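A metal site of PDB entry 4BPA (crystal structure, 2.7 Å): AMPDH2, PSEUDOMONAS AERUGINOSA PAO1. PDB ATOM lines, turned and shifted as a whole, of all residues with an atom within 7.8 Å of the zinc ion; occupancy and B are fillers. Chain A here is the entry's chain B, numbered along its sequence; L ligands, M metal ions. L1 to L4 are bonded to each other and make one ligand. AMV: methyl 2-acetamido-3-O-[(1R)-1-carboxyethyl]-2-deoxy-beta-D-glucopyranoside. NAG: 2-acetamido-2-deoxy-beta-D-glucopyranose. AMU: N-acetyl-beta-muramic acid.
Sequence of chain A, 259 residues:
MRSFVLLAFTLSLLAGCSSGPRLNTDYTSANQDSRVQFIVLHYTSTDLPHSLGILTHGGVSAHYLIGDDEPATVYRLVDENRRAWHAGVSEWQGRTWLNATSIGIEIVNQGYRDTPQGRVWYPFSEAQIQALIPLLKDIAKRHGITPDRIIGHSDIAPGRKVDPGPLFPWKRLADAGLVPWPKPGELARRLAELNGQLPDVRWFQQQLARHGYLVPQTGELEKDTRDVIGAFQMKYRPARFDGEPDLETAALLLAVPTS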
ATOM      1  N   VAL A  40       6.511 -26.729   8.978  1.00  0.00           N
ATOM      2  CA  VAL A  40       7.847 -26.522   9.556  1.00  0.00           C
ATOM      3  C   VAL A  40       8.887 -26.395   8.438  1.00  0.00           C
ATOM      4  O   VAL A  40       9.026 -27.281   7.606  1.00  0.00           O
ATOM      5  CB  VAL A  40       8.252 -27.676  10.490  1.00  0.00           C
ATOM      6  CG1 VAL A  40       9.624 -27.420  11.091  1.00  0.00           C
ATOM      7  CG2 VAL A  40       7.229 -27.841  11.612  1.00  0.00           C
ATOM      8  N   LEU A  41       9.618 -25.284   8.443  1.00  0.00           N
ATOM      9  CA  LEU A  41      10.664 -25.052   7.456  1.00  0.00           C
ATOM     10  C   LEU A  41      12.015 -25.563   7.967  1.00  0.00           C
ATOM     11  O   LEU A  41      12.336 -25.442   9.153  1.00  0.00           O
ATOM     12  CB  LEU A  41      10.763 -23.561   7.123  1.00  0.00           C
ATOM     13  CG  LEU A  41       9.481 -22.905   6.617  1.00  0.00           C
ATOM     14  CD1 LEU A  41       9.660 -21.402   6.502  1.00  0.00           C
ATOM     15  CD2 LEU A  41       9.056 -23.493   5.283  1.00  0.00           C
ATOM     16  N   HIS A  42      12.799 -26.137   7.055  1.00  0.00           N
ATOM     17  CA  HIS A  42      14.136 -26.615   7.372  1.00  0.00           C
ATOM     18  C   HIS A  42      15.107 -26.229   6.285  1.00  0.00           C
ATOM     19  O   HIS A  42      14.709 -25.794   5.199  1.00  0.00           O
ATOM     20  CB  HIS A  42      14.161 -28.147   7.448  1.00  0.00           C
ATOM     21  CG  HIS A  42      13.176 -28.729   8.396  1.00  0.00           C
ATOM     22  ND1 HIS A  42      13.431 -28.866   9.737  1.00  0.00           N
ATOM     23  CD2 HIS A  42      11.935 -29.240   8.200  1.00  0.00           C
ATOM     24  CE1 HIS A  42      12.398 -29.427  10.336  1.00  0.00           C
ATOM     25  NE2 HIS A  42      11.472 -29.671   9.424  1.00  0.00           N
ATOM     26  N   TYR A  43      16.389 -26.368   6.580  1.00  0.00           N
ATOM     27  CA  TYR A  43      17.383 -26.547   5.540  1.00  0.00           C
ATOM     28  C   TYR A  43      17.993 -27.930   5.708  1.00  0.00           C
ATOM     29  O   TYR A  43      17.968 -28.513   6.792  1.00  0.00           O
ATOM     30  CB  TYR A  43      18.444 -25.432   5.499  1.00  0.00           C
ATOM     31  CG  TYR A  43      19.249 -25.167   6.760  1.00  0.00           C
ATOM     32  CD1 TYR A  43      19.987 -26.183   7.372  1.00  0.00           C
ATOM     33  CD2 TYR A  43      19.315 -23.893   7.306  1.00  0.00           C
ATOM     34  CE1 TYR A  43      20.733 -25.941   8.516  1.00  0.00           C
ATOM     35  CE2 TYR A  43      20.059 -23.642   8.447  1.00  0.00           C
ATOM     36  CZ  TYR A  43      20.767 -24.669   9.043  1.00  0.00           C
ATOM     37  OH  TYR A  43      21.505 -24.438  10.192  1.00  0.00           O
ATOM     38  N   THR A  44      18.548 -28.450   4.622  1.00  0.00           N
ATOM     39  CA  THR A  44      19.268 -29.692   4.678  1.00  0.00           C
ATOM     40  C   THR A  44      20.597 -29.085   4.995  1.00  0.00           C
ATOM     41  O   THR A  44      20.788 -27.902   4.691  1.00  0.00           O
ATOM     42  CB  THR A  44      19.375 -30.384   3.311  1.00  0.00           C
ATOM     43  OG1 THR A  44      20.226 -29.612   2.445  1.00  0.00           O
ATOM     44  CG2 THR A  44      18.006 -30.538   2.692  1.00  0.00           C
ATOM     45  N   SER A  45      21.521 -29.815   5.575  1.00  0.00           N
ATOM     46  CA  SER A  45      22.878 -29.267   5.666  1.00  0.00           C
ATOM     47  C   SER A  45      23.766 -29.850   4.560  1.00  0.00           C
ATOM     48  O   SER A  45      24.988 -29.706   4.598  1.00  0.00           O
ATOM     49  CB  SER A  45      23.437 -29.485   7.070  1.00  0.00           C
ATOM     50  OG  SER A  45      22.560 -28.883   8.018  1.00  0.00           O
ATOM     51  N   VAL A  60      15.373 -39.856   8.482  1.00  0.00           N
ATOM     52  CA  VAL A  60      14.654 -38.580   8.488  1.00  0.00           C
ATOM     53  C   VAL A  60      13.943 -38.388   7.153  1.00  0.00           C
ATOM     54  O   VAL A  60      14.356 -38.936   6.126  1.00  0.00           O
ATOM     55  CB  VAL A  60      15.630 -37.412   8.805  1.00  0.00           C
ATOM     56  CG1 VAL A  60      15.030 -36.034   8.531  1.00  0.00           C
ATOM     57  CG2 VAL A  60      16.069 -37.480  10.263  1.00  0.00           C
ATOM     58  N   HIS A  86      10.512 -35.171  10.405  1.00  0.00           N
ATOM     59  CA  HIS A  86      11.356 -33.987  10.227  1.00  0.00           C
ATOM     60  C   HIS A  86      11.550 -33.187  11.520  1.00  0.00           C
ATOM     61  O   HIS A  86      12.615 -32.585  11.730  1.00  0.00           O
ATOM     62  CB  HIS A  86      10.771 -33.072   9.155  1.00  0.00           C
ATOM     63  CG  HIS A  86       9.333 -32.708   9.390  1.00  0.00           C
ATOM     64  ND1 HIS A  86       8.955 -31.539  10.004  1.00  0.00           N
ATOM     65  CD2 HIS A  86       8.199 -33.376   9.101  1.00  0.00           C
ATOM     66  CE1 HIS A  86       7.633 -31.495  10.080  1.00  0.00           C
ATOM     67  NE2 HIS A  86       7.154 -32.599   9.537  1.00  0.00           N
ATOM     68  N   ALA A  87      10.536 -33.191  12.374  1.00  0.00           N
ATOM     69  CA  ALA A  87      10.498 -32.293  13.531  1.00  0.00           C
ATOM     70  C   ALA A  87      11.151 -32.873  14.792  1.00  0.00           C
ATOM     71  O   ALA A  87      11.869 -32.155  15.486  1.00  0.00           O
ATOM     72  CB  ALA A  87       9.051 -31.900  13.819  1.00  0.00           C
ATOM     73  N   ILE A 105       9.134 -29.066   5.223  1.00  0.00           N
ATOM     74  CA  ILE A 105       9.727 -28.648   3.956  1.00  0.00           C
ATOM     75  C   ILE A 105      11.234 -28.414   4.142  1.00  0.00           C
ATOM     76  O   ILE A 105      11.636 -27.494   4.844  1.00  0.00           O
ATOM     77  CB  ILE A 105       9.072 -27.350   3.415  1.00  0.00           C
ATOM     78  CG1 ILE A 105       7.582 -27.548   3.140  1.00  0.00           C
ATOM     79  CG2 ILE A 105       9.770 -26.893   2.140  1.00  0.00           C
ATOM     80  CD1 ILE A 105       6.791 -26.255   3.174  1.00  0.00           C
ATOM     81  N   GLU A 106      12.046 -29.259   3.505  1.00  0.00           N
ATOM     82  CA  GLU A 106      13.492 -29.114   3.545  1.00  0.00           C
ATOM     83  C   GLU A 106      13.930 -28.325   2.333  1.00  0.00           C
ATOM     84  O   GLU A 106      13.287 -28.380   1.285  1.00  0.00           O
ATOM     85  CB  GLU A 106      14.177 -30.488   3.556  1.00  0.00           C
ATOM     86  CG  GLU A 106      13.835 -31.367   4.767  1.00  0.00           C
ATOM     87  CD  GLU A 106      14.884 -31.328   5.882  1.00  0.00           C
ATOM     88  OE1 GLU A 106      15.921 -30.654   5.722  1.00  0.00           O
ATOM     89  OE2 GLU A 106      14.664 -31.998   6.921  1.00  0.00           O
ATOM     90  N   GLY A 152       9.631 -22.065  11.565  1.00  0.00           N
ATOM     91  CA  GLY A 152      10.917 -22.721  11.384  1.00  0.00           C
ATOM     92  C   GLY A 152      11.158 -23.805  12.415  1.00  0.00           C
ATOM     93  O   GLY A 152      10.447 -23.905  13.403  1.00  0.00           O
ATOM     94  N   HIS A 153      12.186 -24.609  12.173  1.00  0.00           N
ATOM     95  CA  HIS A 153      12.546 -25.665  13.103  1.00  0.00           C
ATOM     96  C   HIS A 153      13.159 -25.088  14.370  1.00  0.00           C
ATOM     97  O   HIS A 153      12.966 -25.633  15.467  1.00  0.00           O
ATOM     98  CB  HIS A 153      13.545 -26.612  12.445  1.00  0.00           C
ATOM     99  CG  HIS A 153      13.586 -27.964  13.073  1.00  0.00           C
ATOM    100  ND1 HIS A 153      14.494 -28.927  12.703  1.00  0.00           N
ATOM    101  CD2 HIS A 153      12.834 -28.520  14.056  1.00  0.00           C
ATOM    102  CE1 HIS A 153      14.287 -30.018  13.400  1.00  0.00           C
ATOM    103  NE2 HIS A 153      13.287 -29.796  14.242  1.00  0.00           N
ATOM    104  N   SER A 154      13.897 -23.994  14.209  1.00  0.00           N
ATOM    105  CA  SER A 154      14.460 -23.250  15.338  1.00  0.00           C
ATOM    106  C   SER A 154      13.400 -22.807  16.333  1.00  0.00           C
ATOM    107  O   SER A 154      13.690 -22.679  17.528  1.00  0.00           O
ATOM    108  CB  SER A 154      15.237 -22.041  14.831  1.00  0.00           C
ATOM    109  OG  SER A 154      14.388 -21.135  14.159  1.00  0.00           O
ATOM    110  N   ILE A 156      10.376 -24.460  16.967  1.00  0.00           N
ATOM    111  CA  ILE A 156       9.725 -25.591  17.643  1.00  0.00           C
ATOM    112  C   ILE A 156      10.691 -26.421  18.485  1.00  0.00           C
ATOM    113  O   ILE A 156      10.263 -27.313  19.221  1.00  0.00           O
ATOM    114  CB  ILE A 156       8.947 -26.500  16.650  1.00  0.00           C
ATOM    115  CG1 ILE A 156       9.877 -27.159  15.636  1.00  0.00           C
ATOM    116  CG2 ILE A 156       7.893 -25.690  15.915  1.00  0.00           C
ATOM    117  CD1 ILE A 156       9.216 -28.247  14.826  1.00  0.00           C
ATOM    118  N   LYS A 161      17.698 -26.892  17.718  1.00  0.00           N
ATOM    119  CA  LYS A 161      17.768 -26.615  16.289  1.00  0.00           C
ATOM    120  C   LYS A 161      17.939 -25.145  16.037  1.00  0.00           C
ATOM    121  O   LYS A 161      17.680 -24.312  16.905  1.00  0.00           O
ATOM    122  CB  LYS A 161      16.483 -27.074  15.624  1.00  0.00           C
ATOM    123  CG  LYS A 161      16.230 -28.556  15.745  1.00  0.00           C
ATOM    124  CD  LYS A 161      17.112 -29.337  14.780  1.00  0.00           C
ATOM    125  CE  LYS A 161      16.780 -30.825  14.809  1.00  0.00           C
ATOM    126  NZ  LYS A 161      17.047 -31.569  13.542  1.00  0.00           N
ATOM    127  N   VAL A 162      18.368 -24.820  14.812  1.00  0.00           N
ATOM    128  CA  VAL A 162      18.674 -23.444  14.440  1.00  0.00           C
ATOM    129  C   VAL A 162      18.354 -23.107  12.971  1.00  0.00           C
ATOM    130  O   VAL A 162      18.685 -22.020  12.485  1.00  0.00           O
ATOM    131  CB  VAL A 162      20.145 -23.134  14.791  1.00  0.00           C
ATOM    132  CG1 VAL A 162      21.072 -23.479  13.635  1.00  0.00           C
ATOM    133  CG2 VAL A 162      20.311 -21.679  15.188  1.00  0.00           C
ATOM    134  N   ASP A 163      17.689 -24.034  12.270  1.00  0.00           N
ATOM    135  CA  ASP A 163      17.352 -23.874  10.859  1.00  0.00           C
ATOM    136  C   ASP A 163      15.926 -23.345  10.750  1.00  0.00           C
ATOM    137  O   ASP A 163      15.080 -23.646  11.596  1.00  0.00           O
ATOM    138  CB  ASP A 163      17.489 -25.206  10.113  1.00  0.00           C
ATOM    139  CG  ASP A 163      16.770 -26.345  10.805  1.00  0.00           C
ATOM    140  OD1 ASP A 163      17.057 -26.588  11.993  1.00  0.00           O
ATOM    141  OD2 ASP A 163      15.927 -27.010  10.171  1.00  0.00           O
ATOM    142  N   PRO A 164      15.639 -22.577   9.682  1.00  0.00           N
ATOM    143  CA  PRO A 164      16.525 -22.326   8.543  1.00  0.00           C
ATOM    144  C   PRO A 164      17.544 -21.190   8.721  1.00  0.00           C
ATOM    145  O   PRO A 164      18.212 -20.811   7.745  1.00  0.00           O
ATOM    146  CB  PRO A 164      15.543 -22.022   7.411  1.00  0.00           C
ATOM    147  CG  PRO A 164      14.276 -21.566   8.087  1.00  0.00           C
ATOM    148  CD  PRO A 164      14.380 -21.826   9.557  1.00  0.00           C
HETATM  149  C1  AMV L   1      21.421 -34.356  11.570  1.00  0.00           C
HETATM  150  C2  AMV L   1      20.448 -33.330  10.963  1.00  0.00           C
HETATM  151  C3  AMV L   1      20.554 -31.901  11.640  1.00  0.00           C
HETATM  152  C4  AMV L   1      20.527 -31.962  13.242  1.00  0.00           C
HETATM  153  C5  AMV L   1      20.674 -33.410  13.763  1.00  0.00           C
HETATM  154  C6  AMV L   1      19.342 -34.144  13.829  1.00  0.00           C
HETATM  155  C7  AMV L   1      21.659 -32.884   8.793  1.00  0.00           C
HETATM  156  C8  AMV L   1      21.538 -32.994   7.274  1.00  0.00           C
HETATM  157  C9  AMV L   1      18.362 -31.104  10.278  1.00  0.00           C
HETATM  158  C10 AMV L   1      18.783 -31.020   8.792  1.00  0.00           C
HETATM  159  C11 AMV L   1      17.522 -32.380  10.555  1.00  0.00           C
HETATM  160  O1  AMV L   1      20.893 -35.705  11.381  1.00  0.00           O
HETATM  161  O3  AMV L   1      19.511 -30.931  11.176  1.00  0.00           O
HETATM  162  O4  AMV L   1      21.541 -31.123  13.931  1.00  0.00           O
HETATM  163  O5  AMV L   1      21.661 -34.107  12.966  1.00  0.00           O
HETATM  164  O6  AMV L   1      19.590 -35.242  14.705  1.00  0.00           O
HETATM  165  O7  AMV L   1      22.673 -32.417   9.304  1.00  0.00           O
HETATM  166  O11 AMV L   1      19.636 -30.160   8.503  1.00  0.00           O
HETATM  167  N2  AMV L   1      20.574 -33.312   9.482  1.00  0.00           N
HETATM  168  C12 AMV L   1      21.649 -36.721  12.067  1.00  0.00           C
HETATM  169  OXT AMV L   1      18.223 -31.788   7.973  1.00  0.00           O
HETATM  170  C1  NAG L   2      21.109 -30.002  14.844  1.00  0.00           C
HETATM  171  C2  NAG L   2      21.864 -29.966  16.272  1.00  0.00           C
HETATM  172  C3  NAG L   2      22.029 -28.528  16.943  1.00  0.00           C
HETATM  173  C4  NAG L   2      22.187 -27.372  15.955  1.00  0.00           C
HETATM  174  C5  NAG L   2      21.203 -27.605  14.784  1.00  0.00           C
HETATM  175  C6  NAG L   2      21.316 -26.502  13.763  1.00  0.00           C
HETATM  176  C7  NAG L   2      20.328 -31.581  17.618  1.00  0.00           C
HETATM  177  C8  NAG L   2      19.175 -31.523  16.641  1.00  0.00           C
HETATM  178  N2  NAG L   2      21.456 -30.886  17.382  1.00  0.00           N
HETATM  179  O3  NAG L   2      23.158 -28.557  17.835  1.00  0.00           O
HETATM  180  O4  NAG L   2      21.926 -26.065  16.640  1.00  0.00           O
HETATM  181  O5  NAG L   2      21.462 -28.835  14.101  1.00  0.00           O
HETATM  182  O6  NAG L   2      21.722 -27.078  12.523  1.00  0.00           O
HETATM  183  O7  NAG L   2      20.176 -32.252  18.623  1.00  0.00           O
HETATM  184  C1  AMU L   3      22.672 -25.697  17.886  1.00  0.00           C
HETATM  185  C2  AMU L   3      23.184 -24.254  17.845  1.00  0.00           C
HETATM  186  C3  AMU L   3      23.883 -24.014  19.239  1.00  0.00           C
HETATM  187  C4  AMU L   3      22.672 -23.473  19.998  1.00  0.00           C
HETATM  188  C5  AMU L   3      21.750 -24.733  20.186  1.00  0.00           C
HETATM  189  C6  AMU L   3      20.307 -24.316  20.251  1.00  0.00           C
HETATM  190  C7  AMU L   3      23.831 -22.700  16.051  1.00  0.00           C
HETATM  191  C8  AMU L   3      24.479 -22.572  14.680  1.00  0.00           C
HETATM  192  C9  AMU L   3      26.077 -23.712  20.316  1.00  0.00           C
HETATM  193  C10 AMU L   3      27.459 -24.021  19.708  1.00  0.00           C
HETATM  194  C11 AMU L   3      26.289 -22.725  21.461  1.00  0.00           C
HETATM  195  O3  AMU L   3      25.114 -23.188  19.324  1.00  0.00           O
HETATM  196  O4  AMU L   3      22.918 -22.702  21.246  1.00  0.00           O
HETATM  197  O5  AMU L   3      21.846 -25.818  19.111  1.00  0.00           O
HETATM  198  O6  AMU L   3      20.078 -23.391  19.194  1.00  0.00           O
HETATM  199  O7  AMU L   3      23.354 -21.711  16.610  1.00  0.00           O
HETATM  200  O10 AMU L   3      28.274 -24.607  20.440  1.00  0.00           O
HETATM  201  O11 AMU L   3      27.674 -23.664  18.533  1.00  0.00           O
HETATM  202  N2  AMU L   3      23.886 -23.944  16.584  1.00  0.00           N
HETATM  203  C1  NAG L   4      23.165 -21.231  21.044  1.00  0.00           C
HETATM  204  C2  NAG L   4      22.010 -20.266  21.401  1.00  0.00           C
HETATM  205  C3  NAG L   4      22.359 -18.863  20.878  1.00  0.00           C
HETATM  206  C4  NAG L   4      23.679 -18.371  21.443  1.00  0.00           C
HETATM  207  C5  NAG L   4      24.754 -19.484  21.597  1.00  0.00           C
HETATM  208  C6  NAG L   4      25.768 -19.061  22.651  1.00  0.00           C
HETATM  209  C7  NAG L   4      19.876 -20.466  19.960  1.00  0.00           C
HETATM  210  C8  NAG L   4      20.478 -19.737  18.765  1.00  0.00           C
HETATM  211  N2  NAG L   4      20.625 -20.712  21.078  1.00  0.00           N
HETATM  212  O3  NAG L   4      21.326 -17.938  21.268  1.00  0.00           O
HETATM  213  O4  NAG L   4      24.205 -17.357  20.549  1.00  0.00           O
HETATM  214  O5  NAG L   4      24.199 -20.792  21.930  1.00  0.00           O
HETATM  215  O6  NAG L   4      25.050 -18.891  23.899  1.00  0.00           O
HETATM  216  O7  NAG L   4      18.722 -20.876  19.872  1.00  0.00           O
HETATM  217 ZN    ZN M   1      15.503 -28.967  10.589  1.00  0.00          ZN
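The zinc ion is bound by the side-chain carboxylate of Asp 163 (2.0 Å), a ring nitrogen (ND1) of His 42 (2.2 Å) and a ring nitrogen (ND1) of His 153 (2.3 Å).
N of Ser 45 is in hydrogen-bond range of O11 of AMV L1 (3.5 Å).
The side-chain hydroxyl of Ser 45 lies within hydrogen-bond range of an oxygen (O11) of AMV L1, at 3.2 Å.
The side-chain amino group of Lys 161 lies close to an oxygen (O3) of AMV L1 (3.5 Å).
O11 of AMV L1 lies close to O of Tyr 43 (2.9 Å).
The backbone carbonyl oxygen (O) of Lys 161 is in hydrogen-bond range of an oxygen (O6) of AMU L3 (3.4 Å).
Within 4 Å of the zinc ion: His 42, His 153 and Asp 163.
The nearest printed residue that does not touch the zinc ion is Lys 161 (4.2 Å).
N of His 42 sits at hydrogen-bond distance from O of Ile 105.
O of Asp 163 lies within hydrogen-bond range of N of Ser 154 (2.9 Å).
The backbone NH of His 153 lies within hydrogen-bond range of the backbone carbonyl oxygen of Leu 41, at 3.1 Å.
A ring nitrogen (NE2) of His 42 is in hydrogen-bond range of a ring nitrogen (ND1) of His 86 (3.2 Å).
A ring nitrogen (NE2) of His 153 lies within hydrogen-bond range of the backbone carbonyl oxygen (O) of Ala 87 (3.0 Å).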
